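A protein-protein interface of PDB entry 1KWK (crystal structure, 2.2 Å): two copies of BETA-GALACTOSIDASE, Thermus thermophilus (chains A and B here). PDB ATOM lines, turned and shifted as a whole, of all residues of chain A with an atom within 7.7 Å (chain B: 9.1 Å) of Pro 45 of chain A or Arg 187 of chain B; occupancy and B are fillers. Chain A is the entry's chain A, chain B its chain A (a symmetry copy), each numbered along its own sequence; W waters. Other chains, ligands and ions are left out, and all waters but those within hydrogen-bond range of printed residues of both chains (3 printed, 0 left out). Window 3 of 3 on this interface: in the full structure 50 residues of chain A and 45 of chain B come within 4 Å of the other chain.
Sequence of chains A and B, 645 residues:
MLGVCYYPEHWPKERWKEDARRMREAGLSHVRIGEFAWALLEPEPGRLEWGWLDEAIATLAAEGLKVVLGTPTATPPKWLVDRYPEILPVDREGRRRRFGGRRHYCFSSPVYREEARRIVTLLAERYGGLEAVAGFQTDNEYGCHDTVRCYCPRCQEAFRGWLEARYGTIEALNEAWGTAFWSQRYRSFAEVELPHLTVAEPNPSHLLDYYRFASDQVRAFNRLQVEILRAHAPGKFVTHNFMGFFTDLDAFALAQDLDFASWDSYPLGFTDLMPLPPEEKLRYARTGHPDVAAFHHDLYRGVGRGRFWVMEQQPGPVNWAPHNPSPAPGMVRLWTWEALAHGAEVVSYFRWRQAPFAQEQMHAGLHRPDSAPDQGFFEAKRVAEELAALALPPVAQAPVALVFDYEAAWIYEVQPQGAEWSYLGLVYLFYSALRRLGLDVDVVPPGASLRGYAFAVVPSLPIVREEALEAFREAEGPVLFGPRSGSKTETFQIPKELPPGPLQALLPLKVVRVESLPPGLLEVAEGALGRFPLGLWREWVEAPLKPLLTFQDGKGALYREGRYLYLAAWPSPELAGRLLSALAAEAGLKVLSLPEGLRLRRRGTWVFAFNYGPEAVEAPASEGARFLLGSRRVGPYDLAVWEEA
Water W2 bridges the backbone NH of Lys 78 of chain A (2.9 Å) and the backbone carbonyl oxygen of Arg 185 of chain B (2.9 Å).
Water W1 bridges the guanidinium group of Arg 185 of chain B and the backbone carbonyl oxygen of Pro 43 of chain A.
Water W3 lies within hydrogen-bond range of the side-chain carboxylate of Glu 191 of chain B (3.0 Å), the backbone NH of Trp 79 of chain A (3.3 Å) and the backbone carbonyl oxygen of Arg 185 of chain B (3.3 Å).
No position is printed for both chains.
Of the 8 pairs that touch across the chains among the printed residues, none has its exchanged pair printed and touching as well.
Among the printed residues, pairs that only touch across the chains: Pro 43 of chain A with Arg 187 of chain B (3.4 Å), Trp 79 of chain A with Glu 191 of chain B (3.6 Å), Trp 79 of chain A with Arg 187 of chain B (3.7 Å), Pro 45 of chain A with Arg 187 of chain B (3.8 Å), Ala 39 of chain A with Arg 185 of chain B (3.95 Å) and Asp 82 of chain A with Glu 191 of chain B (3.97 Å).
Of the 15 printed residues of chain A, 7 touch a printed residue of chain B.
Along chain A the printed residues that touch a printed residue of chain B span positions 39 to 82.
Printed residues of chain B that touch a printed residue of chain A: Arg 185, Arg 187 and Glu 191.
Among the printed residues, 8 pairs touch across the chains.
Among the printed residues, Asp or Glu carboxylates within 4 Å of a Lys or Arg side-chain nitrogen of the other chain: Glu 44 of chain A with Arg 187 of chain B.
Printed residues of chain A within 4 Å of Arg 187 of chain B: Pro 43, Glu 44, Pro 45 and Trp 79.
Gly 46 of chain A touches none of the printed residues of chain B.
Printed residues of chain B within 4 Å of Lys 78 of chain A: Glu 191 (2.7 Å).
Printed residues of chain B within 4 Å of Asp 82 of chain A: Glu 191 (3.97 Å).
Printed residues of chain B within 4 Å of Pro 43 of chain A: Arg 187.
Of the printed residues of chain A, Glu 191 of chain B touches Lys 78 (2.7 Å), Trp 79 (3.6 Å) and Asp 82 (3.97 Å).
Of the printed residues of chain A, Arg 185 of chain B touches Ala 39 (3.95 Å).
Ile 170 of chain B touches none of the printed residues of chain A.
OE1 of Glu 44 of chain A is in salt-bridge range of NH1 of Arg 187 of chain B.
The side-chain amino group (NZ) of Lys 78 of chain A lies within hydrogen-bond range of the backbone carbonyl oxygen (O) of Glu 191 of chain B (2.7 Å).
The side-chain carboxylate (OE2) of Glu 191 of chain B lies within salt-bridge range of the guanidinium group (NE) of Arg 187 of chain B (3.1 Å).
The side-chain amino group (NZ) of Lys 78 of chain A lies within salt-bridge range of the side-chain carboxylate (OD2) of Asp 82 of chain A, 2.7 Å away.
The backbone carbonyl oxygen of Thr 179 of chain B sits at hydrogen-bond distance from the backbone NH of Arg 185 of chain B (2.9 Å).
O of Glu 42 of chain A sits at hydrogen-bond distance from NE1 of Trp 79 of chain A.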
ATOM      1  N   ALA A  39      23.285 -20.115 -12.313  1.00  0.00           N
ATOM      2  CA  ALA A  39      23.643 -18.998 -13.186  1.00  0.00           C
ATOM      3  C   ALA A  39      25.008 -18.393 -12.855  1.00  0.00           C
ATOM      4  O   ALA A  39      25.599 -17.698 -13.684  1.00  0.00           O
ATOM      5  CB  ALA A  39      22.567 -17.920 -13.124  1.00  0.00           C
ATOM      6  N   GLU A  42      27.636 -21.295 -14.014  1.00  0.00           N
ATOM      7  CA  GLU A  42      27.665 -21.414 -15.466  1.00  0.00           C
ATOM      8  C   GLU A  42      26.934 -20.236 -16.110  1.00  0.00           C
ATOM      9  O   GLU A  42      25.824 -20.384 -16.623  1.00  0.00           O
ATOM     10  CB  GLU A  42      27.027 -22.741 -15.894  1.00  0.00           C
ATOM     11  CG  GLU A  42      26.948 -22.954 -17.399  1.00  0.00           C
ATOM     12  CD  GLU A  42      26.569 -24.379 -17.772  1.00  0.00           C
ATOM     13  OE1 GLU A  42      25.674 -24.957 -17.120  1.00  0.00           O
ATOM     14  OE2 GLU A  42      27.158 -24.924 -18.729  1.00  0.00           O
ATOM     15  N   PRO A  43      27.552 -19.045 -16.086  1.00  0.00           N
ATOM     16  CA  PRO A  43      26.964 -17.833 -16.668  1.00  0.00           C
ATOM     17  C   PRO A  43      26.812 -17.944 -18.184  1.00  0.00           C
ATOM     18  O   PRO A  43      25.919 -17.337 -18.782  1.00  0.00           O
ATOM     19  CB  PRO A  43      27.946 -16.743 -16.251  1.00  0.00           C
ATOM     20  CG  PRO A  43      29.253 -17.473 -16.206  1.00  0.00           C
ATOM     21  CD  PRO A  43      28.880 -18.760 -15.513  1.00  0.00           C
ATOM     22  N   GLU A  44      27.697 -18.727 -18.793  1.00  0.00           N
ATOM     23  CA  GLU A  44      27.681 -18.965 -20.233  1.00  0.00           C
ATOM     24  C   GLU A  44      27.532 -20.468 -20.445  1.00  0.00           C
ATOM     25  O   GLU A  44      28.134 -21.265 -19.729  1.00  0.00           O
ATOM     26  CB  GLU A  44      28.988 -18.491 -20.881  1.00  0.00           C
ATOM     27  CG  GLU A  44      29.193 -16.982 -20.911  1.00  0.00           C
ATOM     28  CD  GLU A  44      28.126 -16.262 -21.715  1.00  0.00           C
ATOM     29  OE1 GLU A  44      27.830 -16.705 -22.845  1.00  0.00           O
ATOM     30  OE2 GLU A  44      27.589 -15.248 -21.224  1.00  0.00           O
ATOM     31  N   PRO A  45      26.729 -20.875 -21.436  1.00  0.00           N
ATOM     32  CA  PRO A  45      26.505 -22.294 -21.735  1.00  0.00           C
ATOM     33  C   PRO A  45      27.811 -23.064 -21.950  1.00  0.00           C
ATOM     34  O   PRO A  45      28.478 -22.887 -22.970  1.00  0.00           O
ATOM     35  CB  PRO A  45      25.663 -22.251 -23.007  1.00  0.00           C
ATOM     36  CG  PRO A  45      24.935 -20.948 -22.891  1.00  0.00           C
ATOM     37  CD  PRO A  45      26.003 -20.018 -22.388  1.00  0.00           C
ATOM     38  N   GLY A  46      28.173 -23.910 -20.989  1.00  0.00           N
ATOM     39  CA  GLY A  46      29.389 -24.694 -21.120  1.00  0.00           C
ATOM     40  C   GLY A  46      30.610 -24.140 -20.406  1.00  0.00           C
ATOM     41  O   GLY A  46      31.593 -24.857 -20.214  1.00  0.00           O
ATOM     42  N   ARG A  47      30.557 -22.869 -20.015  1.00  0.00           N
ATOM     43  CA  ARG A  47      31.675 -22.238 -19.319  1.00  0.00           C
ATOM     44  C   ARG A  47      31.488 -22.298 -17.807  1.00  0.00           C
ATOM     45  O   ARG A  47      30.770 -21.479 -17.229  1.00  0.00           O
ATOM     46  CB  ARG A  47      31.821 -20.777 -19.765  1.00  0.00           C
ATOM     47  CG  ARG A  47      32.198 -20.607 -21.233  1.00  0.00           C
ATOM     48  CD  ARG A  47      33.566 -21.217 -21.530  1.00  0.00           C
ATOM     49  NE  ARG A  47      33.902 -21.198 -22.955  1.00  0.00           N
ATOM     50  CZ  ARG A  47      34.039 -20.091 -23.682  1.00  0.00           C
ATOM     51  NH1 ARG A  47      33.871 -18.899 -23.124  1.00  0.00           N
ATOM     52  NH2 ARG A  47      34.346 -20.178 -24.971  1.00  0.00           N
ATOM     53  N   LEU A  48      32.143 -23.266 -17.170  1.00  0.00           N
ATOM     54  CA  LEU A  48      32.043 -23.436 -15.725  1.00  0.00           C
ATOM     55  C   LEU A  48      33.040 -22.576 -14.951  1.00  0.00           C
ATOM     56  O   LEU A  48      34.239 -22.578 -15.239  1.00  0.00           O
ATOM     57  CB  LEU A  48      32.252 -24.906 -15.338  1.00  0.00           C
ATOM     58  CG  LEU A  48      31.230 -25.957 -15.781  1.00  0.00           C
ATOM     59  CD1 LEU A  48      29.843 -25.575 -15.285  1.00  0.00           C
ATOM     60  CD2 LEU A  48      31.243 -26.080 -17.292  1.00  0.00           C
ATOM     61  N   PRO A  77      19.397 -21.378 -15.202  1.00  0.00           N
ATOM     62  CA  PRO A  77      19.780 -20.110 -15.846  1.00  0.00           C
ATOM     63  C   PRO A  77      18.838 -19.691 -16.974  1.00  0.00           C
ATOM     64  O   PRO A  77      18.278 -20.533 -17.671  1.00  0.00           O
ATOM     65  CB  PRO A  77      21.192 -20.395 -16.365  1.00  0.00           C
ATOM     66  CG  PRO A  77      21.701 -21.445 -15.424  1.00  0.00           C
ATOM     67  CD  PRO A  77      20.508 -22.344 -15.259  1.00  0.00           C
ATOM     68  N   LYS A  78      18.674 -18.386 -17.159  1.00  0.00           N
ATOM     69  CA  LYS A  78      17.796 -17.887 -18.211  1.00  0.00           C
ATOM     70  C   LYS A  78      18.200 -18.383 -19.599  1.00  0.00           C
ATOM     71  O   LYS A  78      17.334 -18.615 -20.448  1.00  0.00           O
ATOM     72  CB  LYS A  78      17.761 -16.354 -18.191  1.00  0.00           C
ATOM     73  CG  LYS A  78      16.802 -15.720 -19.198  1.00  0.00           C
ATOM     74  CD  LYS A  78      15.421 -16.362 -19.139  1.00  0.00           C
ATOM     75  CE  LYS A  78      14.343 -15.481 -19.760  1.00  0.00           C
ATOM     76  NZ  LYS A  78      14.586 -15.162 -21.194  1.00  0.00           N
ATOM     77  N   TRP A  79      19.502 -18.555 -19.837  1.00  0.00           N
ATOM     78  CA  TRP A  79      19.957 -19.028 -21.144  1.00  0.00           C
ATOM     79  C   TRP A  79      19.535 -20.471 -21.408  1.00  0.00           C
ATOM     80  O   TRP A  79      19.226 -20.834 -22.543  1.00  0.00           O
ATOM     81  CB  TRP A  79      21.482 -18.901 -21.289  1.00  0.00           C
ATOM     82  CG  TRP A  79      22.305 -19.668 -20.282  1.00  0.00           C
ATOM     83  CD1 TRP A  79      22.929 -19.159 -19.180  1.00  0.00           C
ATOM     84  CD2 TRP A  79      22.624 -21.067 -20.313  1.00  0.00           C
ATOM     85  NE1 TRP A  79      23.621 -20.149 -18.525  1.00  0.00           N
ATOM     86  CE2 TRP A  79      23.451 -21.332 -19.198  1.00  0.00           C
ATOM     87  CE3 TRP A  79      22.293 -22.124 -21.174  1.00  0.00           C
ATOM     88  CZ2 TRP A  79      23.953 -22.610 -18.919  1.00  0.00           C
ATOM     89  CZ3 TRP A  79      22.792 -23.398 -20.895  1.00  0.00           C
ATOM     90  CH2 TRP A  79      23.613 -23.626 -19.777  1.00  0.00           C
ATOM     91  N   LEU A  80      19.521 -21.288 -20.360  1.00  0.00           N
ATOM     92  CA  LEU A  80      19.119 -22.683 -20.491  1.00  0.00           C
ATOM     93  C   LEU A  80      17.625 -22.745 -20.785  1.00  0.00           C
ATOM     94  O   LEU A  80      17.173 -23.564 -21.583  1.00  0.00           O
ATOM     95  CB  LEU A  80      19.437 -23.450 -19.205  1.00  0.00           C
ATOM     96  CG  LEU A  80      19.031 -24.925 -19.136  1.00  0.00           C
ATOM     97  CD1 LEU A  80      19.593 -25.681 -20.331  1.00  0.00           C
ATOM     98  CD2 LEU A  80      19.544 -25.530 -17.836  1.00  0.00           C
ATOM     99  N   ASP A  82      15.869 -20.367 -22.238  1.00  0.00           N
ATOM    100  CA  ASP A  82      15.681 -19.856 -23.589  1.00  0.00           C
ATOM    101  C   ASP A  82      16.033 -20.922 -24.622  1.00  0.00           C
ATOM    102  O   ASP A  82      15.382 -21.026 -25.663  1.00  0.00           O
ATOM    103  CB  ASP A  82      16.545 -18.612 -23.813  1.00  0.00           C
ATOM    104  CG  ASP A  82      15.942 -17.362 -23.199  1.00  0.00           C
ATOM    105  OD1 ASP A  82      16.616 -16.312 -23.227  1.00  0.00           O
ATOM    106  OD2 ASP A  82      14.796 -17.426 -22.700  1.00  0.00           O
ATOM    107  N   ARG A  83      17.063 -21.711 -24.331  1.00  0.00           N
ATOM    108  CA  ARG A  83      17.481 -22.769 -25.240  1.00  0.00           C
ATOM    109  C   ARG A  83      16.380 -23.817 -25.368  1.00  0.00           C
ATOM    110  O   ARG A  83      15.923 -24.114 -26.473  1.00  0.00           O
ATOM    111  CB  ARG A  83      18.767 -23.429 -24.737  1.00  0.00           C
ATOM    112  CG  ARG A  83      19.184 -24.653 -25.536  1.00  0.00           C
ATOM    113  CD  ARG A  83      20.558 -25.149 -25.121  1.00  0.00           C
ATOM    114  NE  ARG A  83      21.594 -24.169 -25.427  1.00  0.00           N
ATOM    115  CZ  ARG A  83      22.891 -24.360 -25.220  1.00  0.00           C
ATOM    116  NH1 ARG A  83      23.323 -25.504 -24.703  1.00  0.00           N
ATOM    117  NH2 ARG A  83      23.759 -23.404 -25.530  1.00  0.00           N
ATOM    118  N   ARG A 118      23.664 -33.564 -15.781  1.00  0.00           N
ATOM    119  CA  ARG A 118      24.963 -32.973 -16.079  1.00  0.00           C
ATOM    120  C   ARG A 118      25.524 -32.106 -14.956  1.00  0.00           C
ATOM    121  O   ARG A 118      26.594 -32.395 -14.418  1.00  0.00           O
ATOM    122  CB  ARG A 118      24.884 -32.143 -17.366  1.00  0.00           C
ATOM    123  CG  ARG A 118      26.219 -31.546 -17.802  1.00  0.00           C
ATOM    124  CD  ARG A 118      26.085 -30.817 -19.128  1.00  0.00           C
ATOM    125  NE  ARG A 118      25.212 -29.652 -19.023  1.00  0.00           N
ATOM    126  CZ  ARG A 118      25.535 -28.523 -18.396  1.00  0.00           C
ATOM    127  NH1 ARG A 118      26.720 -28.394 -17.811  1.00  0.00           N
ATOM    128  NH2 ARG A 118      24.665 -27.521 -18.344  1.00  0.00           N
ATOM    129  N   THR B 169      24.452  -0.774 -19.663  1.00  0.00           N
ATOM    130  CA  THR B 169      25.003  -2.122 -19.793  1.00  0.00           C
ATOM    131  C   THR B 169      24.173  -3.124 -18.999  1.00  0.00           C
ATOM    132  O   THR B 169      23.628  -2.797 -17.940  1.00  0.00           O
ATOM    133  CB  THR B 169      26.450  -2.201 -19.272  1.00  0.00           C
ATOM    134  OG1 THR B 169      26.456  -1.998 -17.853  1.00  0.00           O
ATOM    135  CG2 THR B 169      27.318  -1.142 -19.937  1.00  0.00           C
ATOM    136  N   ILE B 170      24.086  -4.349 -19.506  1.00  0.00           N
ATOM    137  CA  ILE B 170      23.321  -5.382 -18.827  1.00  0.00           C
ATOM    138  C   ILE B 170      23.915  -5.619 -17.439  1.00  0.00           C
ATOM    139  O   ILE B 170      23.233  -6.114 -16.540  1.00  0.00           O
ATOM    140  CB  ILE B 170      23.321  -6.705 -19.628  1.00  0.00           C
ATOM    141  CG1 ILE B 170      22.279  -7.666 -19.047  1.00  0.00           C
ATOM    142  CG2 ILE B 170      24.709  -7.345 -19.592  1.00  0.00           C
ATOM    143  CD1 ILE B 170      20.849  -7.181 -19.181  1.00  0.00           C
ATOM    144  N   GLU B 171      25.187  -5.261 -17.273  1.00  0.00           N
ATOM    145  CA  GLU B 171      25.868  -5.422 -15.989  1.00  0.00           C
ATOM    146  C   GLU B 171      25.228  -4.516 -14.941  1.00  0.00           C
ATOM    147  O   GLU B 171      24.981  -4.937 -13.809  1.00  0.00           O
ATOM    148  CB  GLU B 171      27.359  -5.069 -16.101  1.00  0.00           C
ATOM    149  CG  GLU B 171      28.233  -6.086 -16.838  1.00  0.00           C
ATOM    150  CD  GLU B 171      27.942  -6.161 -18.329  1.00  0.00           C
ATOM    151  OE1 GLU B 171      27.864  -5.097 -18.979  1.00  0.00           O
ATOM    152  OE2 GLU B 171      27.805  -7.287 -18.853  1.00  0.00           O
ATOM    153  N   LEU B 173      22.258  -3.403 -14.944  1.00  0.00           N
ATOM    154  CA  LEU B 173      20.913  -3.894 -14.671  1.00  0.00           C
ATOM    155  C   LEU B 173      20.965  -5.084 -13.701  1.00  0.00           C
ATOM    156  O   LEU B 173      20.165  -5.169 -12.767  1.00  0.00           O
ATOM    157  CB  LEU B 173      20.218  -4.291 -15.983  1.00  0.00           C
ATOM    158  CG  LEU B 173      18.788  -4.837 -15.901  1.00  0.00           C
ATOM    159  CD1 LEU B 173      18.090  -4.646 -17.231  1.00  0.00           C
ATOM    160  CD2 LEU B 173      18.811  -6.310 -15.510  1.00  0.00           C
ATOM    161  N   ASN B 174      21.912  -5.993 -13.916  1.00  0.00           N
ATOM    162  CA  ASN B 174      22.045  -7.155 -13.041  1.00  0.00           C
ATOM    163  C   ASN B 174      22.326  -6.731 -11.605  1.00  0.00           C
ATOM    164  O   ASN B 174      21.763  -7.289 -10.662  1.00  0.00           O
ATOM    165  CB  ASN B 174      23.165  -8.081 -13.532  1.00  0.00           C
ATOM    166  CG  ASN B 174      22.762  -8.883 -14.759  1.00  0.00           C
ATOM    167  OD1 ASN B 174      21.713  -9.532 -14.776  1.00  0.00           O
ATOM    168  ND2 ASN B 174      23.597  -8.845 -15.793  1.00  0.00           N
ATOM    169  N   THR B 179      20.266  -9.612  -9.571  1.00  0.00           N
ATOM    170  CA  THR B 179      19.950 -10.858 -10.256  1.00  0.00           C
ATOM    171  C   THR B 179      20.739 -12.100  -9.850  1.00  0.00           C
ATOM    172  O   THR B 179      20.518 -13.182 -10.390  1.00  0.00           O
ATOM    173  CB  THR B 179      20.025 -10.662 -11.777  1.00  0.00           C
ATOM    174  OG1 THR B 179      21.307 -10.131 -12.130  1.00  0.00           O
ATOM    175  CG2 THR B 179      18.936  -9.696 -12.223  1.00  0.00           C
ATOM    176  N   GLN B 184      18.819 -15.327 -11.414  1.00  0.00           N
ATOM    177  CA  GLN B 184      18.076 -14.539 -12.392  1.00  0.00           C
ATOM    178  C   GLN B 184      19.003 -13.834 -13.385  1.00  0.00           C
ATOM    179  O   GLN B 184      18.536 -13.222 -14.344  1.00  0.00           O
ATOM    180  CB  GLN B 184      17.226 -13.486 -11.676  1.00  0.00           C
ATOM    181  CG  GLN B 184      16.131 -14.050 -10.790  1.00  0.00           C
ATOM    182  CD  GLN B 184      15.407 -12.964 -10.011  1.00  0.00           C
ATOM    183  OE1 GLN B 184      14.859 -12.027 -10.591  1.00  0.00           O
ATOM    184  NE2 GLN B 184      15.410 -13.087  -8.688  1.00  0.00           N
ATOM    185  N   ARG B 185      20.310 -13.925 -13.145  1.00  0.00           N
ATOM    186  CA  ARG B 185      21.315 -13.276 -13.982  1.00  0.00           C
ATOM    187  C   ARG B 185      21.020 -13.269 -15.484  1.00  0.00           C
ATOM    188  O   ARG B 185      20.660 -14.294 -16.064  1.00  0.00           O
ATOM    189  CB  ARG B 185      22.686 -13.910 -13.738  1.00  0.00           C
ATOM    190  CG  ARG B 185      23.821 -13.148 -14.394  1.00  0.00           C
ATOM    191  CD  ARG B 185      25.170 -13.797 -14.133  1.00  0.00           C
ATOM    192  NE  ARG B 185      26.250 -13.048 -14.769  1.00  0.00           N
ATOM    193  CZ  ARG B 185      26.362 -12.856 -16.082  1.00  0.00           C
ATOM    194  NH1 ARG B 185      25.459 -13.360 -16.916  1.00  0.00           N
ATOM    195  NH2 ARG B 185      27.379 -12.156 -16.566  1.00  0.00           N
ATOM    196  N   TYR B 186      21.179 -12.099 -16.100  1.00  0.00           N
ATOM    197  CA  TYR B 186      20.943 -11.920 -17.533  1.00  0.00           C
ATOM    198  C   TYR B 186      22.252 -11.688 -18.294  1.00  0.00           C
ATOM    199  O   TYR B 186      23.137 -10.969 -17.822  1.00  0.00           O
ATOM    200  CB  TYR B 186      20.022 -10.722 -17.769  1.00  0.00           C
ATOM    201  CG  TYR B 186      18.632 -10.908 -17.230  1.00  0.00           C
ATOM    202  CD1 TYR B 186      17.769 -11.850 -17.787  1.00  0.00           C
ATOM    203  CD2 TYR B 186      18.180 -10.160 -16.142  1.00  0.00           C
ATOM    204  CE1 TYR B 186      16.486 -12.047 -17.271  1.00  0.00           C
ATOM    205  CE2 TYR B 186      16.905 -10.349 -15.617  1.00  0.00           C
ATOM    206  CZ  TYR B 186      16.062 -11.293 -16.184  1.00  0.00           C
ATOM    207  OH  TYR B 186      14.810 -11.493 -15.657  1.00  0.00           O
ATOM    208  N   ARG B 187      22.364 -12.290 -19.476  1.00  0.00           N
ATOM    209  CA  ARG B 187      23.559 -12.126 -20.301  1.00  0.00           C
ATOM    210  C   ARG B 187      23.432 -10.908 -21.212  1.00  0.00           C
ATOM    211  O   ARG B 187      24.432 -10.344 -21.650  1.00  0.00           O
ATOM    212  CB  ARG B 187      23.801 -13.364 -21.164  1.00  0.00           C
ATOM    213  CG  ARG B 187      24.201 -14.611 -20.401  1.00  0.00           C
ATOM    214  CD  ARG B 187      24.594 -15.692 -21.383  1.00  0.00           C
ATOM    215  NE  ARG B 187      23.503 -16.004 -22.300  1.00  0.00           N
ATOM    216  CZ  ARG B 187      23.673 -16.520 -23.513  1.00  0.00           C
ATOM    217  NH1 ARG B 187      24.898 -16.781 -23.956  1.00  0.00           N
ATOM    218  NH2 ARG B 187      22.621 -16.779 -24.281  1.00  0.00           N
ATOM    219  N   SER B 188      22.196 -10.513 -21.497  1.00  0.00           N
ATOM    220  CA  SER B 188      21.934  -9.368 -22.361  1.00  0.00           C
ATOM    221  C   SER B 188      20.489  -8.910 -22.203  1.00  0.00           C
ATOM    222  O   SER B 188      19.642  -9.656 -21.716  1.00  0.00           O
ATOM    223  CB  SER B 188      22.177  -9.745 -23.822  1.00  0.00           C
ATOM    224  OG  SER B 188      21.242 -10.722 -24.250  1.00  0.00           O
ATOM    225  N   PHE B 189      20.211  -7.680 -22.623  1.00  0.00           N
ATOM    226  CA  PHE B 189      18.859  -7.142 -22.531  1.00  0.00           C
ATOM    227  C   PHE B 189      17.884  -8.025 -23.305  1.00  0.00           C
ATOM    228  O   PHE B 189      16.698  -8.087 -22.987  1.00  0.00           O
ATOM    229  CB  PHE B 189      18.827  -5.713 -23.080  1.00  0.00           C
ATOM    230  CG  PHE B 189      19.609  -4.734 -22.254  1.00  0.00           C
ATOM    231  CD1 PHE B 189      19.152  -4.342 -20.996  1.00  0.00           C
ATOM    232  CD2 PHE B 189      20.813  -4.216 -22.721  1.00  0.00           C
ATOM    233  CE1 PHE B 189      19.882  -3.450 -20.216  1.00  0.00           C
ATOM    234  CE2 PHE B 189      21.551  -3.324 -21.950  1.00  0.00           C
ATOM    235  CZ  PHE B 189      21.086  -2.940 -20.696  1.00  0.00           C
ATOM    236  N   ALA B 190      18.397  -8.715 -24.318  1.00  0.00           N
ATOM    237  CA  ALA B 190      17.567  -9.590 -25.135  1.00  0.00           C
ATOM    238  C   ALA B 190      16.978 -10.732 -24.307  1.00  0.00           C
ATOM    239  O   ALA B 190      15.944 -11.291 -24.665  1.00  0.00           O
ATOM    240  CB  ALA B 190      18.387 -10.149 -26.300  1.00  0.00           C
ATOM    241  N   GLU B 191      17.635 -11.080 -23.203  1.00  0.00           N
ATOM    242  CA  GLU B 191      17.152 -12.162 -22.348  1.00  0.00           C
ATOM    243  C   GLU B 191      16.072 -11.729 -21.352  1.00  0.00           C
ATOM    244  O   GLU B 191      15.381 -12.574 -20.778  1.00  0.00           O
ATOM    245  CB  GLU B 191      18.309 -12.804 -21.575  1.00  0.00           C
ATOM    246  CG  GLU B 191      19.330 -13.520 -22.444  1.00  0.00           C
ATOM    247  CD  GLU B 191      20.208 -14.468 -21.648  1.00  0.00           C
ATOM    248  OE1 GLU B 191      20.667 -14.084 -20.552  1.00  0.00           O
ATOM    249  OE2 GLU B 191      20.446 -15.597 -22.123  1.00  0.00           O
ATOM    250  N   VAL B 192      15.927 -10.424 -21.144  1.00  0.00           N
ATOM    251  CA  VAL B 192      14.929  -9.920 -20.210  1.00  0.00           C
ATOM    252  C   VAL B 192      13.533  -9.920 -20.820  1.00  0.00           C
ATOM    253  O   VAL B 192      13.328  -9.438 -21.936  1.00  0.00           O
ATOM    254  CB  VAL B 192      15.255  -8.482 -19.752  1.00  0.00           C
ATOM    255  CG1 VAL B 192      14.226  -8.018 -18.731  1.00  0.00           C
ATOM    256  CG2 VAL B 192      16.648  -8.429 -19.159  1.00  0.00           C
HETATM  257  O   HOH W   1      23.993 -15.856 -17.053  1.00  0.00           O
HETATM  258  O   HOH W   2      20.065 -16.940 -15.127  1.00  0.00           O
HETATM  259  O   HOH W   3      21.510 -16.193 -18.655  1.00  0.00           O
